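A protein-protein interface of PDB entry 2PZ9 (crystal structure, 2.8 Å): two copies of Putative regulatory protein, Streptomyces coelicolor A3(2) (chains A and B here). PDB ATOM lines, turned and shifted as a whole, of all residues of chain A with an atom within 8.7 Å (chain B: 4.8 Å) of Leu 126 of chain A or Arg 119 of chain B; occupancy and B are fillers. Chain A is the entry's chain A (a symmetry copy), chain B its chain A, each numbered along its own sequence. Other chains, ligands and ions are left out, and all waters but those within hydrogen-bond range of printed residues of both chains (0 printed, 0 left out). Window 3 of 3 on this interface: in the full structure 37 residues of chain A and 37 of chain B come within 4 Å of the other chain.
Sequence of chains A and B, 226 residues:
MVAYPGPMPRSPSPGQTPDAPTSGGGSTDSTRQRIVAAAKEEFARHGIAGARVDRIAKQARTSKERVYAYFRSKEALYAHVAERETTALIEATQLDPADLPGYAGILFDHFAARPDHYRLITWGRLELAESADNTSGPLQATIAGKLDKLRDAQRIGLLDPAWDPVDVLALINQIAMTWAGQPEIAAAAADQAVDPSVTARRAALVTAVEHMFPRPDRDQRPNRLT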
ATOM      1  N   ILE A  48     -10.336 -32.817   1.490  1.00  0.00           N
ATOM      2  CA  ILE A  48      -9.718 -32.664   0.155  1.00  0.00           C
ATOM      3  C   ILE A  48      -8.582 -33.663  -0.124  1.00  0.00           C
ATOM      4  O   ILE A  48      -8.708 -34.500  -1.014  1.00  0.00           O
ATOM      5  CB  ILE A  48      -9.172 -31.238  -0.062  1.00  0.00           C
ATOM      6  CG1 ILE A  48     -10.244 -30.192   0.238  1.00  0.00           C
ATOM      7  CG2 ILE A  48      -8.564 -31.100  -1.480  1.00  0.00           C
ATOM      8  CD1 ILE A  48      -9.665 -28.890   0.710  1.00  0.00           C
ATOM      9  N   TYR A  78     -13.455 -29.214  -5.297  1.00  0.00           N
ATOM     10  CA  TYR A  78     -13.789 -28.721  -3.961  1.00  0.00           C
ATOM     11  C   TYR A  78     -14.304 -27.276  -4.027  1.00  0.00           C
ATOM     12  O   TYR A  78     -15.434 -27.006  -3.598  1.00  0.00           O
ATOM     13  CB  TYR A  78     -12.637 -28.840  -2.950  1.00  0.00           C
ATOM     14  CG  TYR A  78     -13.043 -28.344  -1.551  1.00  0.00           C
ATOM     15  CD1 TYR A  78     -12.745 -27.031  -1.120  1.00  0.00           C
ATOM     16  CD2 TYR A  78     -13.746 -29.181  -0.663  1.00  0.00           C
ATOM     17  CE1 TYR A  78     -13.127 -26.575   0.145  1.00  0.00           C
ATOM     18  CE2 TYR A  78     -14.132 -28.735   0.617  1.00  0.00           C
ATOM     19  CZ  TYR A  78     -13.824 -27.434   1.011  1.00  0.00           C
ATOM     20  OH  TYR A  78     -14.228 -26.997   2.275  1.00  0.00           O
ATOM     21  N   ARG A 119     -19.190 -30.408   8.023  1.00  0.00           N
ATOM     22  CA  ARG A 119     -17.950 -31.180   7.861  1.00  0.00           C
ATOM     23  C   ARG A 119     -17.142 -30.610   6.729  1.00  0.00           C
ATOM     24  O   ARG A 119     -15.941 -30.384   6.847  1.00  0.00           O
ATOM     25  CB  ARG A 119     -18.241 -32.614   7.469  1.00  0.00           C
ATOM     26  CG  ARG A 119     -18.875 -33.469   8.498  1.00  0.00           C
ATOM     27  CD  ARG A 119     -18.329 -34.852   8.302  1.00  0.00           C
ATOM     28  NE  ARG A 119     -17.414 -35.196   9.384  1.00  0.00           N
ATOM     29  CZ  ARG A 119     -16.355 -36.004   9.297  1.00  0.00           C
ATOM     30  NH1 ARG A 119     -15.994 -36.575   8.152  1.00  0.00           N
ATOM     31  NH2 ARG A 119     -15.637 -36.233  10.386  1.00  0.00           N
ATOM     32  N   LEU A 120     -17.825 -30.391   5.620  1.00  0.00           N
ATOM     33  CA  LEU A 120     -17.178 -29.929   4.414  1.00  0.00           C
ATOM     34  C   LEU A 120     -16.543 -28.535   4.531  1.00  0.00           C
ATOM     35  O   LEU A 120     -15.426 -28.344   4.030  1.00  0.00           O
ATOM     36  CB  LEU A 120     -18.118 -30.064   3.213  1.00  0.00           C
ATOM     37  CG  LEU A 120     -17.682 -29.518   1.870  1.00  0.00           C
ATOM     38  CD1 LEU A 120     -18.415 -30.239   0.795  1.00  0.00           C
ATOM     39  CD2 LEU A 120     -18.035 -28.050   1.824  1.00  0.00           C
ATOM     40  N   ILE A 121     -17.187 -27.571   5.186  1.00  0.00           N
ATOM     41  CA  ILE A 121     -16.440 -26.321   5.348  1.00  0.00           C
ATOM     42  C   ILE A 121     -15.333 -26.390   6.383  1.00  0.00           C
ATOM     43  O   ILE A 121     -14.287 -25.744   6.220  1.00  0.00           O
ATOM     44  CB  ILE A 121     -17.280 -25.029   5.525  1.00  0.00           C
ATOM     45  CG1 ILE A 121     -18.186 -25.116   6.757  1.00  0.00           C
ATOM     46  CG2 ILE A 121     -17.940 -24.613   4.145  1.00  0.00           C
ATOM     47  CD1 ILE A 121     -19.215 -23.994   6.858  1.00  0.00           C
ATOM     48  N   THR A 122     -15.548 -27.188   7.427  1.00  0.00           N
ATOM     49  CA  THR A 122     -14.522 -27.376   8.464  1.00  0.00           C
ATOM     50  C   THR A 122     -13.241 -27.985   7.879  1.00  0.00           C
ATOM     51  O   THR A 122     -12.150 -27.533   8.184  1.00  0.00           O
ATOM     52  CB  THR A 122     -15.027 -28.258   9.620  1.00  0.00           C
ATOM     53  OG1 THR A 122     -16.325 -27.815  10.027  1.00  0.00           O
ATOM     54  CG2 THR A 122     -14.069 -28.202  10.800  1.00  0.00           C
ATOM     55  N   TRP A 123     -13.373 -29.002   7.036  1.00  0.00           N
ATOM     56  CA  TRP A 123     -12.217 -29.526   6.333  1.00  0.00           C
ATOM     57  C   TRP A 123     -11.465 -28.411   5.629  1.00  0.00           C
ATOM     58  O   TRP A 123     -10.242 -28.359   5.674  1.00  0.00           O
ATOM     59  CB  TRP A 123     -12.654 -30.505   5.286  1.00  0.00           C
ATOM     60  CG  TRP A 123     -13.019 -31.826   5.776  1.00  0.00           C
ATOM     61  CD1 TRP A 123     -14.274 -32.351   5.835  1.00  0.00           C
ATOM     62  CD2 TRP A 123     -12.127 -32.856   6.239  1.00  0.00           C
ATOM     63  NE1 TRP A 123     -14.226 -33.649   6.308  1.00  0.00           N
ATOM     64  CE2 TRP A 123     -12.921 -33.986   6.557  1.00  0.00           C
ATOM     65  CE3 TRP A 123     -10.737 -32.940   6.407  1.00  0.00           C
ATOM     66  CZ2 TRP A 123     -12.373 -35.178   7.039  1.00  0.00           C
ATOM     67  CZ3 TRP A 123     -10.193 -34.127   6.885  1.00  0.00           C
ATOM     68  CH2 TRP A 123     -11.014 -35.227   7.198  1.00  0.00           C
ATOM     69  N   GLY A 124     -12.211 -27.523   4.977  1.00  0.00           N
ATOM     70  CA  GLY A 124     -11.630 -26.424   4.230  1.00  0.00           C
ATOM     71  C   GLY A 124     -10.930 -25.399   5.093  1.00  0.00           C
ATOM     72  O   GLY A 124      -9.926 -24.831   4.675  1.00  0.00           O
ATOM     73  N   ARG A 125     -11.448 -25.135   6.286  1.00  0.00           N
ATOM     74  CA  ARG A 125     -10.785 -24.155   7.154  1.00  0.00           C
ATOM     75  C   ARG A 125      -9.391 -24.637   7.526  1.00  0.00           C
ATOM     76  O   ARG A 125      -8.411 -23.908   7.374  1.00  0.00           O
ATOM     77  CB  ARG A 125     -11.603 -23.871   8.403  1.00  0.00           C
ATOM     78  CG  ARG A 125     -13.047 -23.603   8.084  1.00  0.00           C
ATOM     79  CD  ARG A 125     -13.723 -22.855   9.169  1.00  0.00           C
ATOM     80  NE  ARG A 125     -15.158 -23.116   9.122  1.00  0.00           N
ATOM     81  CZ  ARG A 125     -16.085 -22.411   9.769  1.00  0.00           C
ATOM     82  NH1 ARG A 125     -15.747 -21.367  10.518  1.00  0.00           N
ATOM     83  NH2 ARG A 125     -17.364 -22.748   9.646  1.00  0.00           N
ATOM     84  N   LEU A 126      -9.324 -25.894   7.953  1.00  0.00           N
ATOM     85  CA  LEU A 126      -8.082 -26.567   8.316  1.00  0.00           C
ATOM     86  C   LEU A 126      -7.143 -26.886   7.157  1.00  0.00           C
ATOM     87  O   LEU A 126      -5.931 -26.723   7.276  1.00  0.00           O
ATOM     88  CB  LEU A 126      -8.392 -27.866   9.054  1.00  0.00           C
ATOM     89  CG  LEU A 126      -9.086 -27.761  10.414  1.00  0.00           C
ATOM     90  CD1 LEU A 126      -9.732 -29.093  10.719  1.00  0.00           C
ATOM     91  CD2 LEU A 126      -8.140 -27.344  11.547  1.00  0.00           C
ATOM     92  N   GLU A 127      -7.685 -27.372   6.049  1.00  0.00           N
ATOM     93  CA  GLU A 127      -6.825 -27.785   4.942  1.00  0.00           C
ATOM     94  C   GLU A 127      -6.240 -26.592   4.136  1.00  0.00           C
ATOM     95  O   GLU A 127      -5.100 -26.657   3.695  1.00  0.00           O
ATOM     96  CB  GLU A 127      -7.520 -28.809   4.037  1.00  0.00           C
ATOM     97  CG  GLU A 127      -7.884 -30.095   4.721  1.00  0.00           C
ATOM     98  CD  GLU A 127      -7.976 -31.267   3.767  1.00  0.00           C
ATOM     99  OE1 GLU A 127      -7.041 -31.429   2.957  1.00  0.00           O
ATOM    100  OE2 GLU A 127      -8.961 -32.044   3.827  1.00  0.00           O
ATOM    101  N   LEU A 128      -6.993 -25.505   3.973  1.00  0.00           N
ATOM    102  CA  LEU A 128      -6.517 -24.342   3.215  1.00  0.00           C
ATOM    103  C   LEU A 128      -5.989 -23.222   4.129  1.00  0.00           C
ATOM    104  O   LEU A 128      -4.771 -22.965   4.147  1.00  0.00           O
ATOM    105  CB  LEU A 128      -7.607 -23.843   2.263  1.00  0.00           C
ATOM    106  CG  LEU A 128      -8.202 -25.006   1.446  1.00  0.00           C
ATOM    107  CD1 LEU A 128      -9.682 -24.767   1.142  1.00  0.00           C
ATOM    108  CD2 LEU A 128      -7.392 -25.353   0.165  1.00  0.00           C
ATOM    109  N   ALA A 129      -6.890 -22.579   4.884  1.00  0.00           N
ATOM    110  CA  ALA A 129      -6.537 -21.490   5.834  1.00  0.00           C
ATOM    111  C   ALA A 129      -5.416 -20.503   5.397  1.00  0.00           C
ATOM    112  O   ALA A 129      -5.471 -19.870   4.329  1.00  0.00           O
ATOM    113  N   ALA B  44      -1.319 -30.081  14.625  1.00  0.00           N
ATOM    114  CA  ALA B  44      -2.116 -28.891  14.394  1.00  0.00           C
ATOM    115  C   ALA B  44      -2.066 -28.458  12.919  1.00  0.00           C
ATOM    116  O   ALA B  44      -3.083 -28.094  12.347  1.00  0.00           O
ATOM    117  CB  ALA B  44      -1.692 -27.758  15.323  1.00  0.00           C
ATOM    118  N   ARG B  45      -0.886 -28.526  12.310  1.00  0.00           N
ATOM    119  CA  ARG B  45      -0.694 -28.193  10.902  1.00  0.00           C
ATOM    120  C   ARG B  45      -1.413 -29.122   9.942  1.00  0.00           C
ATOM    121  O   ARG B  45      -2.198 -28.691   9.118  1.00  0.00           O
ATOM    122  CB  ARG B  45       0.790 -28.248  10.568  1.00  0.00           C
ATOM    123  CG  ARG B  45       1.404 -26.936  10.184  1.00  0.00           C
ATOM    124  CD  ARG B  45       2.922 -27.055  10.164  1.00  0.00           C
ATOM    125  NE  ARG B  45       3.552 -25.779  10.501  1.00  0.00           N
ATOM    126  CZ  ARG B  45       3.648 -25.282  11.737  1.00  0.00           C
ATOM    127  NH1 ARG B  45       3.150 -25.943  12.786  1.00  0.00           N
ATOM    128  NH2 ARG B  45       4.232 -24.104  11.929  1.00  0.00           N
ATOM    129  N   PRO B 115      -3.717 -21.613  20.139  1.00  0.00           N
ATOM    130  CA  PRO B 115      -4.538 -21.669  18.936  1.00  0.00           C
ATOM    131  C   PRO B 115      -4.532 -23.070  18.352  1.00  0.00           C
ATOM    132  O   PRO B 115      -5.542 -23.543  17.824  1.00  0.00           O
ATOM    133  CB  PRO B 115      -3.823 -20.712  17.972  1.00  0.00           C
ATOM    134  CG  PRO B 115      -3.035 -19.816  18.827  1.00  0.00           C
ATOM    135  CD  PRO B 115      -2.634 -20.615  20.013  1.00  0.00           C
ATOM    136  N   ASP B 116      -3.393 -23.733  18.474  1.00  0.00           N
ATOM    137  CA  ASP B 116      -3.185 -25.022  17.851  1.00  0.00           C
ATOM    138  C   ASP B 116      -3.716 -26.231  18.655  1.00  0.00           C
ATOM    139  O   ASP B 116      -3.752 -27.348  18.136  1.00  0.00           O
ATOM    140  CB  ASP B 116      -1.709 -25.168  17.498  1.00  0.00           C
ATOM    141  CG  ASP B 116      -0.807 -25.116  18.720  1.00  0.00           C
ATOM    142  OD1 ASP B 116      -1.262 -24.700  19.825  1.00  0.00           O
ATOM    143  OD2 ASP B 116       0.378 -25.511  18.561  1.00  0.00           O
ATOM    144  N   HIS B 117      -4.140 -26.016  19.900  1.00  0.00           N
ATOM    145  CA  HIS B 117      -4.858 -27.061  20.629  1.00  0.00           C
ATOM    146  C   HIS B 117      -6.165 -27.215  19.901  1.00  0.00           C
ATOM    147  O   HIS B 117      -6.644 -28.337  19.659  1.00  0.00           O
ATOM    148  CB  HIS B 117      -5.117 -26.667  22.094  1.00  0.00           C
ATOM    149  CG  HIS B 117      -5.994 -27.633  22.858  1.00  0.00           C
ATOM    150  ND1 HIS B 117      -5.842 -27.865  24.215  1.00  0.00           N
ATOM    151  CD2 HIS B 117      -7.033 -28.419  22.463  1.00  0.00           C
ATOM    152  CE1 HIS B 117      -6.745 -28.747  24.620  1.00  0.00           C
ATOM    153  NE2 HIS B 117      -7.478 -29.103  23.574  1.00  0.00           N
ATOM    154  N   TYR B 118      -6.728 -26.069  19.541  1.00  0.00           N
ATOM    155  CA  TYR B 118      -7.987 -26.051  18.842  1.00  0.00           C
ATOM    156  C   TYR B 118      -7.918 -26.786  17.487  1.00  0.00           C
ATOM    157  O   TYR B 118      -8.774 -27.629  17.198  1.00  0.00           O
ATOM    158  CB  TYR B 118      -8.489 -24.622  18.673  1.00  0.00           C
ATOM    159  CG  TYR B 118      -9.800 -24.587  17.938  1.00  0.00           C
ATOM    160  CD1 TYR B 118     -10.999 -24.819  18.610  1.00  0.00           C
ATOM    161  CD2 TYR B 118      -9.846 -24.375  16.553  1.00  0.00           C
ATOM    162  CE1 TYR B 118     -12.213 -24.805  17.942  1.00  0.00           C
ATOM    163  CE2 TYR B 118     -11.062 -24.374  15.870  1.00  0.00           C
ATOM    164  CZ  TYR B 118     -12.240 -24.583  16.580  1.00  0.00           C
ATOM    165  OH  TYR B 118     -13.447 -24.566  15.919  1.00  0.00           O
ATOM    166  N   ARG B 119      -6.902 -26.464  16.681  1.00  0.00           N
ATOM    167  CA  ARG B 119      -6.660 -27.133  15.395  1.00  0.00           C
ATOM    168  C   ARG B 119      -6.531 -28.615  15.611  1.00  0.00           C
ATOM    169  O   ARG B 119      -7.133 -29.421  14.910  1.00  0.00           O
ATOM    170  CB  ARG B 119      -5.343 -26.696  14.786  1.00  0.00           C
ATOM    171  CG  ARG B 119      -5.267 -25.299  14.300  1.00  0.00           C
ATOM    172  CD  ARG B 119      -4.376 -25.313  13.094  1.00  0.00           C
ATOM    173  NE  ARG B 119      -5.158 -25.098  11.882  1.00  0.00           N
ATOM    174  CZ  ARG B 119      -4.885 -25.584  10.669  1.00  0.00           C
ATOM    175  NH1 ARG B 119      -3.843 -26.378  10.444  1.00  0.00           N
ATOM    176  NH2 ARG B 119      -5.688 -25.273   9.663  1.00  0.00           N
ATOM    177  N   LEU B 120      -5.719 -28.959  16.594  1.00  0.00           N
ATOM    178  CA  LEU B 120      -5.416 -30.344  16.874  1.00  0.00           C
ATOM    179  C   LEU B 120      -6.627 -31.178  17.318  1.00  0.00           C
ATOM    180  O   LEU B 120      -6.764 -32.322  16.863  1.00  0.00           O
ATOM    181  CB  LEU B 120      -4.225 -30.453  17.830  1.00  0.00           C
ATOM    182  CG  LEU B 120      -3.822 -31.815  18.353  1.00  0.00           C
ATOM    183  CD1 LEU B 120      -2.387 -31.777  18.743  1.00  0.00           C
ATOM    184  CD2 LEU B 120      -4.666 -32.119  19.568  1.00  0.00           C
ATOM    185  N   ILE B 121      -7.515 -30.652  18.160  1.00  0.00           N
ATOM    186  CA  ILE B 121      -8.694 -31.482  18.420  1.00  0.00           C
ATOM    187  C   ILE B 121      -9.689 -31.523  17.274  1.00  0.00           C
ATOM    188  O   ILE B 121     -10.336 -32.556  17.049  1.00  0.00           O
ATOM    189  CB  ILE B 121      -9.420 -31.252  19.772  1.00  0.00           C
ATOM    190  CG1 ILE B 121      -9.911 -29.807  19.903  1.00  0.00           C
ATOM    191  CG2 ILE B 121      -8.565 -31.858  20.961  1.00  0.00           C
ATOM    192  CD1 ILE B 121     -10.412 -29.441  21.297  1.00  0.00           C
ATOM    193  N   THR B 122      -9.790 -30.417  16.540  1.00  0.00           N
ATOM    194  CA  THR B 122     -10.681 -30.361  15.371  1.00  0.00           C
ATOM    195  C   THR B 122     -10.275 -31.391  14.309  1.00  0.00           C
ATOM    196  O   THR B 122     -11.122 -32.081  13.766  1.00  0.00           O
ATOM    197  CB  THR B 122     -10.711 -28.958  14.737  1.00  0.00           C
ATOM    198  OG1 THR B 122     -10.880 -27.975  15.762  1.00  0.00           O
ATOM    199  CG2 THR B 122     -11.840 -28.847  13.725  1.00  0.00           C
ATOM    200  N   TRP B 123      -8.984 -31.502  14.020  1.00  0.00           N
ATOM    201  CA  TRP B 123      -8.518 -32.555  13.139  1.00  0.00           C
ATOM    202  C   TRP B 123      -9.024 -33.908  13.603  1.00  0.00           C
ATOM    203  O   TRP B 123      -9.468 -34.718  12.798  1.00  0.00           O
ATOM    204  CB  TRP B 123      -7.019 -32.607  13.151  1.00  0.00           C
ATOM    205  CG  TRP B 123      -6.350 -31.582  12.363  1.00  0.00           C
ATOM    206  CD1 TRP B 123      -5.649 -30.519  12.844  1.00  0.00           C
ATOM    207  CD2 TRP B 123      -6.247 -31.519  10.929  1.00  0.00           C
ATOM    208  NE1 TRP B 123      -5.112 -29.790  11.800  1.00  0.00           N
ATOM    209  CE2 TRP B 123      -5.458 -30.385  10.615  1.00  0.00           C
ATOM    210  CE3 TRP B 123      -6.735 -32.312   9.880  1.00  0.00           C
ATOM    211  CZ2 TRP B 123      -5.152 -30.022   9.300  1.00  0.00           C
ATOM    212  CZ3 TRP B 123      -6.430 -31.951   8.573  1.00  0.00           C
ATOM    213  CH2 TRP B 123      -5.649 -30.812   8.298  1.00  0.00           C
ATOM    214  N   LEU B 126     -12.941 -34.698  13.014  1.00  0.00           N
ATOM    215  CA  LEU B 126     -13.120 -35.059  11.613  1.00  0.00           C
ATOM    216  C   LEU B 126     -12.416 -36.338  11.167  1.00  0.00           C
ATOM    217  O   LEU B 126     -12.981 -37.129  10.417  1.00  0.00           O
ATOM    218  CB  LEU B 126     -12.649 -33.916  10.718  1.00  0.00           C
ATOM    219  CG  LEU B 126     -13.421 -32.596  10.789  1.00  0.00           C
ATOM    220  CD1 LEU B 126     -12.532 -31.500  10.247  1.00  0.00           C
ATOM    221  CD2 LEU B 126     -14.758 -32.634  10.037  1.00  0.00           C
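Of the 12 printed residues of chain B, 4 touch a printed residue of chain A.
Printed residues of chain B that touch a printed residue of chain A: Arg 119, Thr 122, Trp 123 and Leu 126.
Hydrophobic or aromatic side chains of chain B that line the printed part of chain A: Trp 123 and Leu 126.
Of the 13 printed residues of chain A, 5 touch a printed residue of chain B.
Printed residues of chain A that touch a printed residue of chain B: Arg 119, Thr 122, Trp 123, Arg 125 and Leu 126.
Hydrophobic or aromatic side chains of chain A within 4 Å of the printed part of chain B: Trp 123 and Leu 126.
Arg 119 of chain B touches just these residues of chain A: Arg 125 (3.8 Å) and Leu 126 (2.8 Å).
Thr 122 of chain B touches just these residues of chain A: Thr 122 (3.7 Å) and Leu 126 (3.7 Å).
Printed residues of chain B within 4 Å of Arg 125 of chain A: Arg 119 (3.8 Å).
Printed residues of chain A within 4 Å of Trp 123 of chain B: Leu 126.
Gly 124 of chain A touches none of the printed residues of chain B.
Ala 129 of chain A touches none of the printed residues of chain B.
The nearest residue of chain A that does not touch Arg 119 of chain B is Glu 127 of chain A (4.6 Å).
The nearest printed residue of chain B that does not touch Trp 123 of chain A is Trp 123 of chain B (4.7 Å).
Arg 119 of chain A touches Leu 126 of chain B, and with the chains exchanged Leu 126 of chain A touches Arg 119 of chain B.
Thr 122 of chain A touches Leu 126 of chain B, and with the chains exchanged Leu 126 of chain A touches Thr 122 of chain B.
Trp 123 of chain A touches Leu 126 of chain B, and with the chains exchanged Leu 126 of chain A touches Trp 123 of chain B.
Leu 126 of chain A touches its own counterpart, Leu 126 of chain B.
6 positions are printed for both chains.
Of the 9 pairs that touch across the chains among the printed residues, 8 have their exchanged pair printed and touching as well.
NH2 of Arg 119 of chain B lies within hydrogen-bond range of O of Leu 126 of chain A (2.8 Å).
O of Leu 126 of chain B is in hydrogen-bond range of NH2 of Arg 119 of chain A, at 2.8 Å.
Among the printed residues, pairs that only touch across the chains: Leu 126 of chain A with Thr 122 of chain B (3.7 Å), Thr 122 of chain A with Leu 126 of chain B (3.7 Å), Leu 126 of chain A with Leu 126 of chain B (3.7 Å), Thr 122 of chain A with Thr 122 of chain B (3.7 Å), Arg 125 of chain A with Arg 119 of chain B (3.8 Å), Trp 123 of chain A with Leu 126 of chain B (3.9 Å) and Leu 126 of chain A with Trp 123 of chain B (3.9 Å).
The guanidinium group of Arg 119 of chain B lies within hydrogen-bond range of the backbone carbonyl oxygen of Ala 44 of chain B, at 2.7 Å.
The backbone carbonyl oxygen of Ala 44 of chain B sits at hydrogen-bond distance from the indole nitrogen of Trp 123 of chain B, 2.7 Å away.
O of Arg 45 of chain B is in hydrogen-bond range of NH1 of Arg 119 of chain B.
The backbone carbonyl oxygen of Tyr 118 of chain B sits at hydrogen-bond distance from the side-chain hydroxyl of Thr 122 of chain B (2.6 Å).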
